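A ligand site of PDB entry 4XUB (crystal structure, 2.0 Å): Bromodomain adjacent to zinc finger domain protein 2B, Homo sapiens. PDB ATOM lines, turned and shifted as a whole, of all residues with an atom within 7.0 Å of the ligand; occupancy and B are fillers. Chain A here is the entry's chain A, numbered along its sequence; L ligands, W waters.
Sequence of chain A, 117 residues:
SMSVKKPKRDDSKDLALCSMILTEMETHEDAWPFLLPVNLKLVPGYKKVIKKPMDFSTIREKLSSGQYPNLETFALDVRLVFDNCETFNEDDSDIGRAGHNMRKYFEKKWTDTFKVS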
ATOM      1  N   ALA A  31     -11.952  12.863  -8.638  1.00  0.00           N
ATOM      2  CA  ALA A  31     -12.008  14.240  -9.117  1.00  0.00           C
ATOM      3  C   ALA A  31     -11.749  15.283  -8.030  1.00  0.00           C
ATOM      4  O   ALA A  31     -11.568  16.465  -8.364  1.00  0.00           O
ATOM      5  CB  ALA A  31     -13.336  14.540  -9.782  1.00  0.00           C
ATOM      6  N   TRP A  32     -11.751  14.879  -6.769  1.00  0.00           N
ATOM      7  CA  TRP A  32     -11.661  15.825  -5.646  1.00  0.00           C
ATOM      8  C   TRP A  32     -10.490  16.808  -5.704  1.00  0.00           C
ATOM      9  O   TRP A  32     -10.660  17.941  -5.308  1.00  0.00           O
ATOM     10  CB  TRP A  32     -11.761  15.124  -4.274  1.00  0.00           C
ATOM     11  CG  TRP A  32     -10.684  14.157  -4.044  1.00  0.00           C
ATOM     12  CD1 TRP A  32     -10.725  12.836  -4.338  1.00  0.00           C
ATOM     13  CD2 TRP A  32      -9.388  14.416  -3.503  1.00  0.00           C
ATOM     14  NE1 TRP A  32      -9.533  12.252  -4.040  1.00  0.00           N
ATOM     15  CE2 TRP A  32      -8.682  13.194  -3.532  1.00  0.00           C
ATOM     16  CE3 TRP A  32      -8.736  15.574  -3.021  1.00  0.00           C
ATOM     17  CZ2 TRP A  32      -7.365  13.074  -3.069  1.00  0.00           C
ATOM     18  CZ3 TRP A  32      -7.423  15.450  -2.571  1.00  0.00           C
ATOM     19  CH2 TRP A  32      -6.755  14.205  -2.598  1.00  0.00           C
ATOM     20  N   PRO A  33      -9.312  16.417  -6.246  1.00  0.00           N
ATOM     21  CA  PRO A  33      -8.298  17.458  -6.257  1.00  0.00           C
ATOM     22  C   PRO A  33      -8.583  18.594  -7.239  1.00  0.00           C
ATOM     23  O   PRO A  33      -7.858  19.583  -7.206  1.00  0.00           O
ATOM     24  CB  PRO A  33      -7.015  16.707  -6.657  1.00  0.00           C
ATOM     25  CG  PRO A  33      -7.299  15.242  -6.472  1.00  0.00           C
ATOM     26  CD  PRO A  33      -8.780  15.138  -6.755  1.00  0.00           C
ATOM     27  N   PHE A  34      -9.573  18.403  -8.129  1.00  0.00           N
ATOM     28  CA  PHE A  34      -9.692  19.200  -9.339  1.00  0.00           C
ATOM     29  C   PHE A  34     -10.979  19.985  -9.432  1.00  0.00           C
ATOM     30  O   PHE A  34     -11.209  20.665 -10.444  1.00  0.00           O
ATOM     31  CB  PHE A  34      -9.595  18.292 -10.580  1.00  0.00           C
ATOM     32  CG  PHE A  34      -8.426  17.391 -10.560  1.00  0.00           C
ATOM     33  CD1 PHE A  34      -7.131  17.918 -10.737  1.00  0.00           C
ATOM     34  CD2 PHE A  34      -8.570  16.040 -10.369  1.00  0.00           C
ATOM     35  CE1 PHE A  34      -6.022  17.125 -10.643  1.00  0.00           C
ATOM     36  CE2 PHE A  34      -7.438  15.219 -10.298  1.00  0.00           C
ATOM     37  CZ  PHE A  34      -6.175  15.758 -10.468  1.00  0.00           C
ATOM     38  N   LEU A  35     -11.850  19.868  -8.428  1.00  0.00           N
ATOM     39  CA  LEU A  35     -13.178  20.435  -8.515  1.00  0.00           C
ATOM     40  C   LEU A  35     -13.195  21.963  -8.423  1.00  0.00           C
ATOM     41  O   LEU A  35     -14.071  22.616  -9.019  1.00  0.00           O
ATOM     42  CB  LEU A  35     -14.092  19.875  -7.433  1.00  0.00           C
ATOM     43  CG  LEU A  35     -14.302  18.361  -7.470  1.00  0.00           C
ATOM     44  CD1 LEU A  35     -15.169  17.930  -6.283  1.00  0.00           C
ATOM     45  CD2 LEU A  35     -14.938  17.933  -8.783  1.00  0.00           C
ATOM     46  N   LEU A  36     -12.260  22.535  -7.649  1.00  0.00           N
ATOM     47  CA  LEU A  36     -12.190  23.985  -7.427  1.00  0.00           C
ATOM     48  C   LEU A  36     -10.750  24.473  -7.712  1.00  0.00           C
ATOM     49  O   LEU A  36      -9.811  23.686  -7.669  1.00  0.00           O
ATOM     50  CB  LEU A  36     -12.592  24.301  -5.986  1.00  0.00           C
ATOM     51  CG  LEU A  36     -13.985  23.938  -5.473  1.00  0.00           C
ATOM     52  CD1 LEU A  36     -14.094  24.205  -3.977  1.00  0.00           C
ATOM     53  CD2 LEU A  36     -15.045  24.727  -6.224  1.00  0.00           C
ATOM     54  N   PRO A  37     -10.582  25.777  -7.982  1.00  0.00           N
ATOM     55  CA  PRO A  37      -9.194  26.240  -8.170  1.00  0.00           C
ATOM     56  C   PRO A  37      -8.287  25.957  -6.955  1.00  0.00           C
ATOM     57  O   PRO A  37      -8.759  25.979  -5.815  1.00  0.00           O
ATOM     58  CB  PRO A  37      -9.329  27.763  -8.406  1.00  0.00           C
ATOM     59  CG  PRO A  37     -10.784  28.037  -8.586  1.00  0.00           C
ATOM     60  CD  PRO A  37     -11.563  26.871  -8.014  1.00  0.00           C
ATOM     61  N   VAL A  38      -7.007  25.657  -7.186  1.00  0.00           N
ATOM     62  CA  VAL A  38      -6.084  25.594  -6.046  1.00  0.00           C
ATOM     63  C   VAL A  38      -6.059  26.944  -5.368  1.00  0.00           C
ATOM     64  O   VAL A  38      -5.927  27.989  -6.010  1.00  0.00           O
ATOM     65  CB  VAL A  38      -4.667  25.176  -6.470  1.00  0.00           C
ATOM     66  CG1 VAL A  38      -3.728  25.151  -5.253  1.00  0.00           C
ATOM     67  CG2 VAL A  38      -4.693  23.813  -7.159  1.00  0.00           C
ATOM     68  N   ASN A  39      -6.262  26.926  -4.062  1.00  0.00           N
ATOM     69  CA  ASN A  39      -6.284  28.118  -3.255  1.00  0.00           C
ATOM     70  C   ASN A  39      -4.861  28.669  -3.067  1.00  0.00           C
ATOM     71  O   ASN A  39      -4.047  28.061  -2.388  1.00  0.00           O
ATOM     72  CB  ASN A  39      -6.936  27.788  -1.891  1.00  0.00           C
ATOM     73  CG  ASN A  39      -7.129  29.016  -1.013  1.00  0.00           C
ATOM     74  OD1 ASN A  39      -6.329  29.939  -1.023  1.00  0.00           O
ATOM     75  ND2 ASN A  39      -8.169  29.002  -0.213  1.00  0.00           N
ATOM     76  N   LEU A  40      -4.587  29.828  -3.634  1.00  0.00           N
ATOM     77  CA  LEU A  40      -3.234  30.374  -3.681  1.00  0.00           C
ATOM     78  C   LEU A  40      -2.743  30.893  -2.348  1.00  0.00           C
ATOM     79  O   LEU A  40      -1.563  31.198  -2.232  1.00  0.00           O
ATOM     80  CB  LEU A  40      -3.101  31.474  -4.746  1.00  0.00           C
ATOM     81  CG  LEU A  40      -3.514  31.105  -6.192  1.00  0.00           C
ATOM     82  CD1 LEU A  40      -3.320  32.325  -7.099  1.00  0.00           C
ATOM     83  CD2 LEU A  40      -2.789  29.868  -6.738  1.00  0.00           C
ATOM     84  N   LEU A  42      -3.587  28.892   0.414  1.00  0.00           N
ATOM     85  CA  LEU A  42      -3.378  27.633   1.108  1.00  0.00           C
ATOM     86  C   LEU A  42      -2.162  26.879   0.630  1.00  0.00           C
ATOM     87  O   LEU A  42      -1.633  26.076   1.396  1.00  0.00           O
ATOM     88  CB  LEU A  42      -4.574  26.694   0.942  1.00  0.00           C
ATOM     89  CG  LEU A  42      -5.467  26.407   2.154  1.00  0.00           C
ATOM     90  CD1 LEU A  42      -5.822  27.671   2.942  1.00  0.00           C
ATOM     91  CD2 LEU A  42      -6.727  25.697   1.662  1.00  0.00           C
ATOM     92  N   VAL A  43      -1.742  27.079  -0.619  1.00  0.00           N
ATOM     93  CA  VAL A  43      -0.734  26.198  -1.170  1.00  0.00           C
ATOM     94  C   VAL A  43       0.570  26.922  -1.483  1.00  0.00           C
ATOM     95  O   VAL A  43       0.615  27.613  -2.502  1.00  0.00           O
ATOM     96  CB  VAL A  43      -1.272  25.441  -2.399  1.00  0.00           C
ATOM     97  CG1 VAL A  43      -0.285  24.394  -2.866  1.00  0.00           C
ATOM     98  CG2 VAL A  43      -2.589  24.770  -2.058  1.00  0.00           C
ATOM     99  N   TYR A  46       2.292  27.496  -5.358  1.00  0.00           N
ATOM    100  CA  TYR A  46       1.402  27.289  -6.523  1.00  0.00           C
ATOM    101  C   TYR A  46       1.388  28.448  -7.491  1.00  0.00           C
ATOM    102  O   TYR A  46       1.566  28.288  -8.715  1.00  0.00           O
ATOM    103  CB  TYR A  46      -0.052  26.987  -6.106  1.00  0.00           C
ATOM    104  CG  TYR A  46      -0.671  26.131  -7.165  1.00  0.00           C
ATOM    105  CD1 TYR A  46      -0.391  24.774  -7.233  1.00  0.00           C
ATOM    106  CD2 TYR A  46      -1.418  26.703  -8.181  1.00  0.00           C
ATOM    107  CE1 TYR A  46      -0.938  23.973  -8.244  1.00  0.00           C
ATOM    108  CE2 TYR A  46      -1.967  25.923  -9.181  1.00  0.00           C
ATOM    109  CZ  TYR A  46      -1.722  24.571  -9.210  1.00  0.00           C
ATOM    110  OH  TYR A  46      -2.272  23.820 -10.233  1.00  0.00           O
ATOM    111  N   MET A  54      -5.851  25.867 -13.858  1.00  0.00           N
ATOM    112  CA  MET A  54      -7.117  25.458 -14.401  1.00  0.00           C
ATOM    113  C   MET A  54      -7.709  24.373 -13.509  1.00  0.00           C
ATOM    114  O   MET A  54      -6.955  23.683 -12.807  1.00  0.00           O
ATOM    115  CB  MET A  54      -6.950  25.003 -15.851  1.00  0.00           C
ATOM    116  CG  MET A  54      -8.259  24.704 -16.568  1.00  0.00           C
ATOM    117  SD  MET A  54      -9.429  26.070 -16.552  1.00  0.00           S
ATOM    118  CE  MET A  54      -8.360  27.393 -17.188  1.00  0.00           C
ATOM    119  N   ASP A  55      -9.031  24.235 -13.535  1.00  0.00           N
ATOM    120  CA  ASP A  55      -9.764  23.251 -12.711  1.00  0.00           C
ATOM    121  C   ASP A  55     -11.165  23.022 -13.304  1.00  0.00           C
ATOM    122  O   ASP A  55     -11.624  23.810 -14.125  1.00  0.00           O
ATOM    123  CB  ASP A  55      -9.943  23.740 -11.288  1.00  0.00           C
ATOM    124  CG  ASP A  55     -10.942  24.867 -11.194  1.00  0.00           C
ATOM    125  OD1 ASP A  55     -10.594  25.985 -11.637  1.00  0.00           O
ATOM    126  OD2 ASP A  55     -12.070  24.638 -10.701  1.00  0.00           O
ATOM    127  N   VAL A  81      -5.260  21.026 -16.744  1.00  0.00           N
ATOM    128  CA  VAL A  81      -5.512  20.583 -15.363  1.00  0.00           C
ATOM    129  C   VAL A  81      -4.518  19.460 -14.978  1.00  0.00           C
ATOM    130  O   VAL A  81      -3.847  19.527 -13.949  1.00  0.00           O
ATOM    131  CB  VAL A  81      -6.954  20.058 -15.181  1.00  0.00           C
ATOM    132  CG1 VAL A  81      -7.135  19.495 -13.767  1.00  0.00           C
ATOM    133  CG2 VAL A  81      -8.004  21.137 -15.371  1.00  0.00           C
ATOM    134  N   ASN A  84      -0.644  20.584 -15.104  1.00  0.00           N
ATOM    135  CA  ASN A  84      -0.332  21.335 -13.876  1.00  0.00           C
ATOM    136  C   ASN A  84      -0.176  20.407 -12.697  1.00  0.00           C
ATOM    137  O   ASN A  84       0.729  20.579 -11.883  1.00  0.00           O
ATOM    138  CB  ASN A  84      -1.428  22.321 -13.567  1.00  0.00           C
ATOM    139  CG  ASN A  84      -1.460  23.520 -14.509  1.00  0.00           C
ATOM    140  OD1 ASN A  84      -0.521  23.786 -15.252  1.00  0.00           O
ATOM    141  ND2 ASN A  84      -2.566  24.272 -14.458  1.00  0.00           N
ATOM    142  N   CYS A  85      -1.062  19.422 -12.608  1.00  0.00           N
ATOM    143  CA  CYS A  85      -1.040  18.491 -11.495  1.00  0.00           C
ATOM    144  C   CYS A  85       0.271  17.727 -11.467  1.00  0.00           C
ATOM    145  O   CYS A  85       0.868  17.546 -10.415  1.00  0.00           O
ATOM    146  CB  CYS A  85      -2.225  17.527 -11.566  1.00  0.00           C
ATOM    147  SG  CYS A  85      -2.387  16.351 -10.217  1.00  0.00           S
ATOM    148  N   PHE A  88       3.241  19.925 -10.347  1.00  0.00           N
ATOM    149  CA  PHE A  88       3.279  20.358  -8.952  1.00  0.00           C
ATOM    150  C   PHE A  88       3.346  19.198  -7.969  1.00  0.00           C
ATOM    151  O   PHE A  88       3.904  19.361  -6.892  1.00  0.00           O
ATOM    152  CB  PHE A  88       2.095  21.269  -8.644  1.00  0.00           C
ATOM    153  CG  PHE A  88       2.273  22.093  -7.402  1.00  0.00           C
ATOM    154  CD1 PHE A  88       3.063  23.247  -7.422  1.00  0.00           C
ATOM    155  CD2 PHE A  88       1.671  21.732  -6.226  1.00  0.00           C
ATOM    156  CE1 PHE A  88       3.234  24.020  -6.286  1.00  0.00           C
ATOM    157  CE2 PHE A  88       1.836  22.495  -5.071  1.00  0.00           C
ATOM    158  CZ  PHE A  88       2.633  23.640  -5.099  1.00  0.00           C
ATOM    159  N   ASN A  89       2.768  18.053  -8.324  1.00  0.00           N
ATOM    160  CA  ASN A  89       2.654  16.929  -7.396  1.00  0.00           C
ATOM    161  C   ASN A  89       3.515  15.720  -7.784  1.00  0.00           C
ATOM    162  O   ASN A  89       3.673  15.400  -8.955  1.00  0.00           O
ATOM    163  CB  ASN A  89       1.202  16.480  -7.328  1.00  0.00           C
ATOM    164  CG  ASN A  89       0.275  17.597  -6.897  1.00  0.00           C
ATOM    165  OD1 ASN A  89       0.070  17.806  -5.708  1.00  0.00           O
ATOM    166  ND2 ASN A  89      -0.285  18.326  -7.871  1.00  0.00           N
ATOM    167  N   ILE A  95      -2.820  12.988  -4.740  1.00  0.00           N
ATOM    168  CA  ILE A  95      -3.180  13.940  -5.775  1.00  0.00           C
ATOM    169  C   ILE A  95      -2.505  13.599  -7.092  1.00  0.00           C
ATOM    170  O   ILE A  95      -3.159  13.698  -8.130  1.00  0.00           O
ATOM    171  CB  ILE A  95      -2.779  15.390  -5.399  1.00  0.00           C
ATOM    172  CG1 ILE A  95      -3.644  15.886  -4.240  1.00  0.00           C
ATOM    173  CG2 ILE A  95      -2.962  16.316  -6.592  1.00  0.00           C
ATOM    174  CD1 ILE A  95      -3.075  17.118  -3.563  1.00  0.00           C
HETATM  175  C1  LIG L   1      -9.335  24.332  -2.673  1.00  0.00           C
HETATM  176  C2  LIG L   1      -7.951  24.015  -2.105  1.00  0.00           C
HETATM  177  C3  LIG L   1      -7.651  23.162  -1.130  1.00  0.00           C
HETATM  178  N1  LIG L   1      -6.816  24.577  -2.539  1.00  0.00           N
HETATM  179  N2  LIG L   1      -5.833  24.085  -1.840  1.00  0.00           N
HETATM  180  N3  LIG L   1      -6.312  23.215  -0.997  1.00  0.00           N
HETATM  181  C4  LIG L   1      -5.348  22.522  -0.090  1.00  0.00           C
HETATM  182  C5  LIG L   1      -5.188  21.002  -0.401  1.00  0.00           C
HETATM  183  N4  LIG L   1      -4.407  20.872  -1.703  1.00  0.00           N
HETATM  184  C6  LIG L   1      -3.078  20.878  -1.722  1.00  0.00           C
HETATM  185  N5  LIG L   1      -2.639  20.782  -2.993  1.00  0.00           N
HETATM  186  C7  LIG L   1      -3.733  20.772  -3.784  1.00  0.00           C
HETATM  187  C8  LIG L   1      -3.604  20.607  -5.145  1.00  0.00           C
HETATM  188  C9  LIG L   1      -4.521  20.039  -5.931  1.00  0.00           C
HETATM  189  C10 LIG L   1      -2.519  20.860  -5.882  1.00  0.00           C
HETATM  190  N6  LIG L   1      -2.766  20.489  -7.156  1.00  0.00           N
HETATM  191  N7  LIG L   1      -4.029  19.980  -7.152  1.00  0.00           N
HETATM  192  C11 LIG L   1      -4.699  19.442  -8.329  1.00  0.00           C
HETATM  193  C12 LIG L   1      -4.830  20.812  -2.989  1.00  0.00           C
HETATM  194  C13 LIG L   1      -6.155  20.811  -3.381  1.00  0.00           C
HETATM  195  C14 LIG L   1      -6.589  21.765  -4.296  1.00  0.00           C
HETATM  196  C15 LIG L   1      -7.888  21.848  -4.763  1.00  0.00           C
HETATM  197  C16 LIG L   1      -8.821  20.967  -4.292  1.00  0.00           C
HETATM  198  C17 LIG L   1     -10.143  20.995  -4.716  1.00  0.00           C
HETATM  199  N8  LIG L   1     -11.309  21.039  -5.106  1.00  0.00           N
HETATM  200  C18 LIG L   1      -8.440  19.991  -3.326  1.00  0.00           C
HETATM  201  C19 LIG L   1      -7.114  19.938  -2.867  1.00  0.00           C
HETATM  202  O   HOH W   1     -11.900  26.402  -2.093  1.00  0.00           O
HETATM  203  O   HOH W   2      -2.192  21.236 -10.011  1.00  0.00           O
HETATM  204  O   HOH W   3      -5.253  17.540  -0.266  1.00  0.00           O
HETATM  205  O   HOH W   4      -0.236  19.946  -3.820  1.00  0.00           O
HETATM  206  O   HOH W   5      -7.602  18.166   0.090  1.00  0.00           O
HETATM  207  O   HOH W   6     -12.543  18.426  -3.606  1.00  0.00           O
HETATM  208  O   HOH W   7      -2.778  22.578   1.841  1.00  0.00           O
HETATM  209  O   HOH W   8     -14.217  20.571  -3.563  1.00  0.00           O
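The backbone NH (N) of Asn 39 lies within hydrogen-bond range of a nitrogen (N1) of the ligand, at 2.9 Å. The backbone NH (N) of Leu 36 lies within hydrogen-bond range of a nitrogen (N8) of the ligand (3.1 Å). The side-chain amide nitrogen (ND2) of Asn 89 is in hydrogen-bond range of a nitrogen (N6) of the ligand.
OD1 of Asn 39 sits at hydrogen-bond distance from N of Leu 42 (3.3 Å). The side-chain amide nitrogen of Asn 89 lies within hydrogen-bond range of the backbone carbonyl oxygen of Cys 85 (2.9 Å). The side-chain sulfur (SG) of Cys 85 is in hydrogen-bond range of the backbone carbonyl oxygen (O) of Ile 95.
The backbone carbonyl oxygen of Trp 32 lies close to a nitrogen (N8) of the ligand, 3.2 Å away. O of Pro 33 touches C15 of the ligand (3.3 Å). Phe 34 touches the ligand (CE1 to C11, 3.5 Å). N of Leu 35 touches N8 of the ligand, 3.6 Å away. O of Pro 37 touches C1 of the ligand, 3.6 Å away. Val 38 touches the ligand. Leu 42 touches the ligand. Val 43 touches the ligand. Ile 95 touches the ligand. Hydrophobic or aromatic side chains within 4 Å of the ligand: Pro 33, Phe 34, Leu 35, Leu 36, Val 38, Leu 42, Val 43 and Ile 95.
Water W4 lies within hydrogen-bond range of N5 of the ligand (2.7 Å) and OD1 of Asn 89 (2.9 Å). Water W2 lies within hydrogen-bond range of the side-chain hydroxyl (OH) of Tyr 46 (2.6 Å), a nitrogen (N6) of the ligand (3.0 Å) and the backbone NH (N) of Cys 85 (3.4 Å). Water W6 bridges O of Trp 32 (2.6 Å) and N8 of the ligand (3.3 Å).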
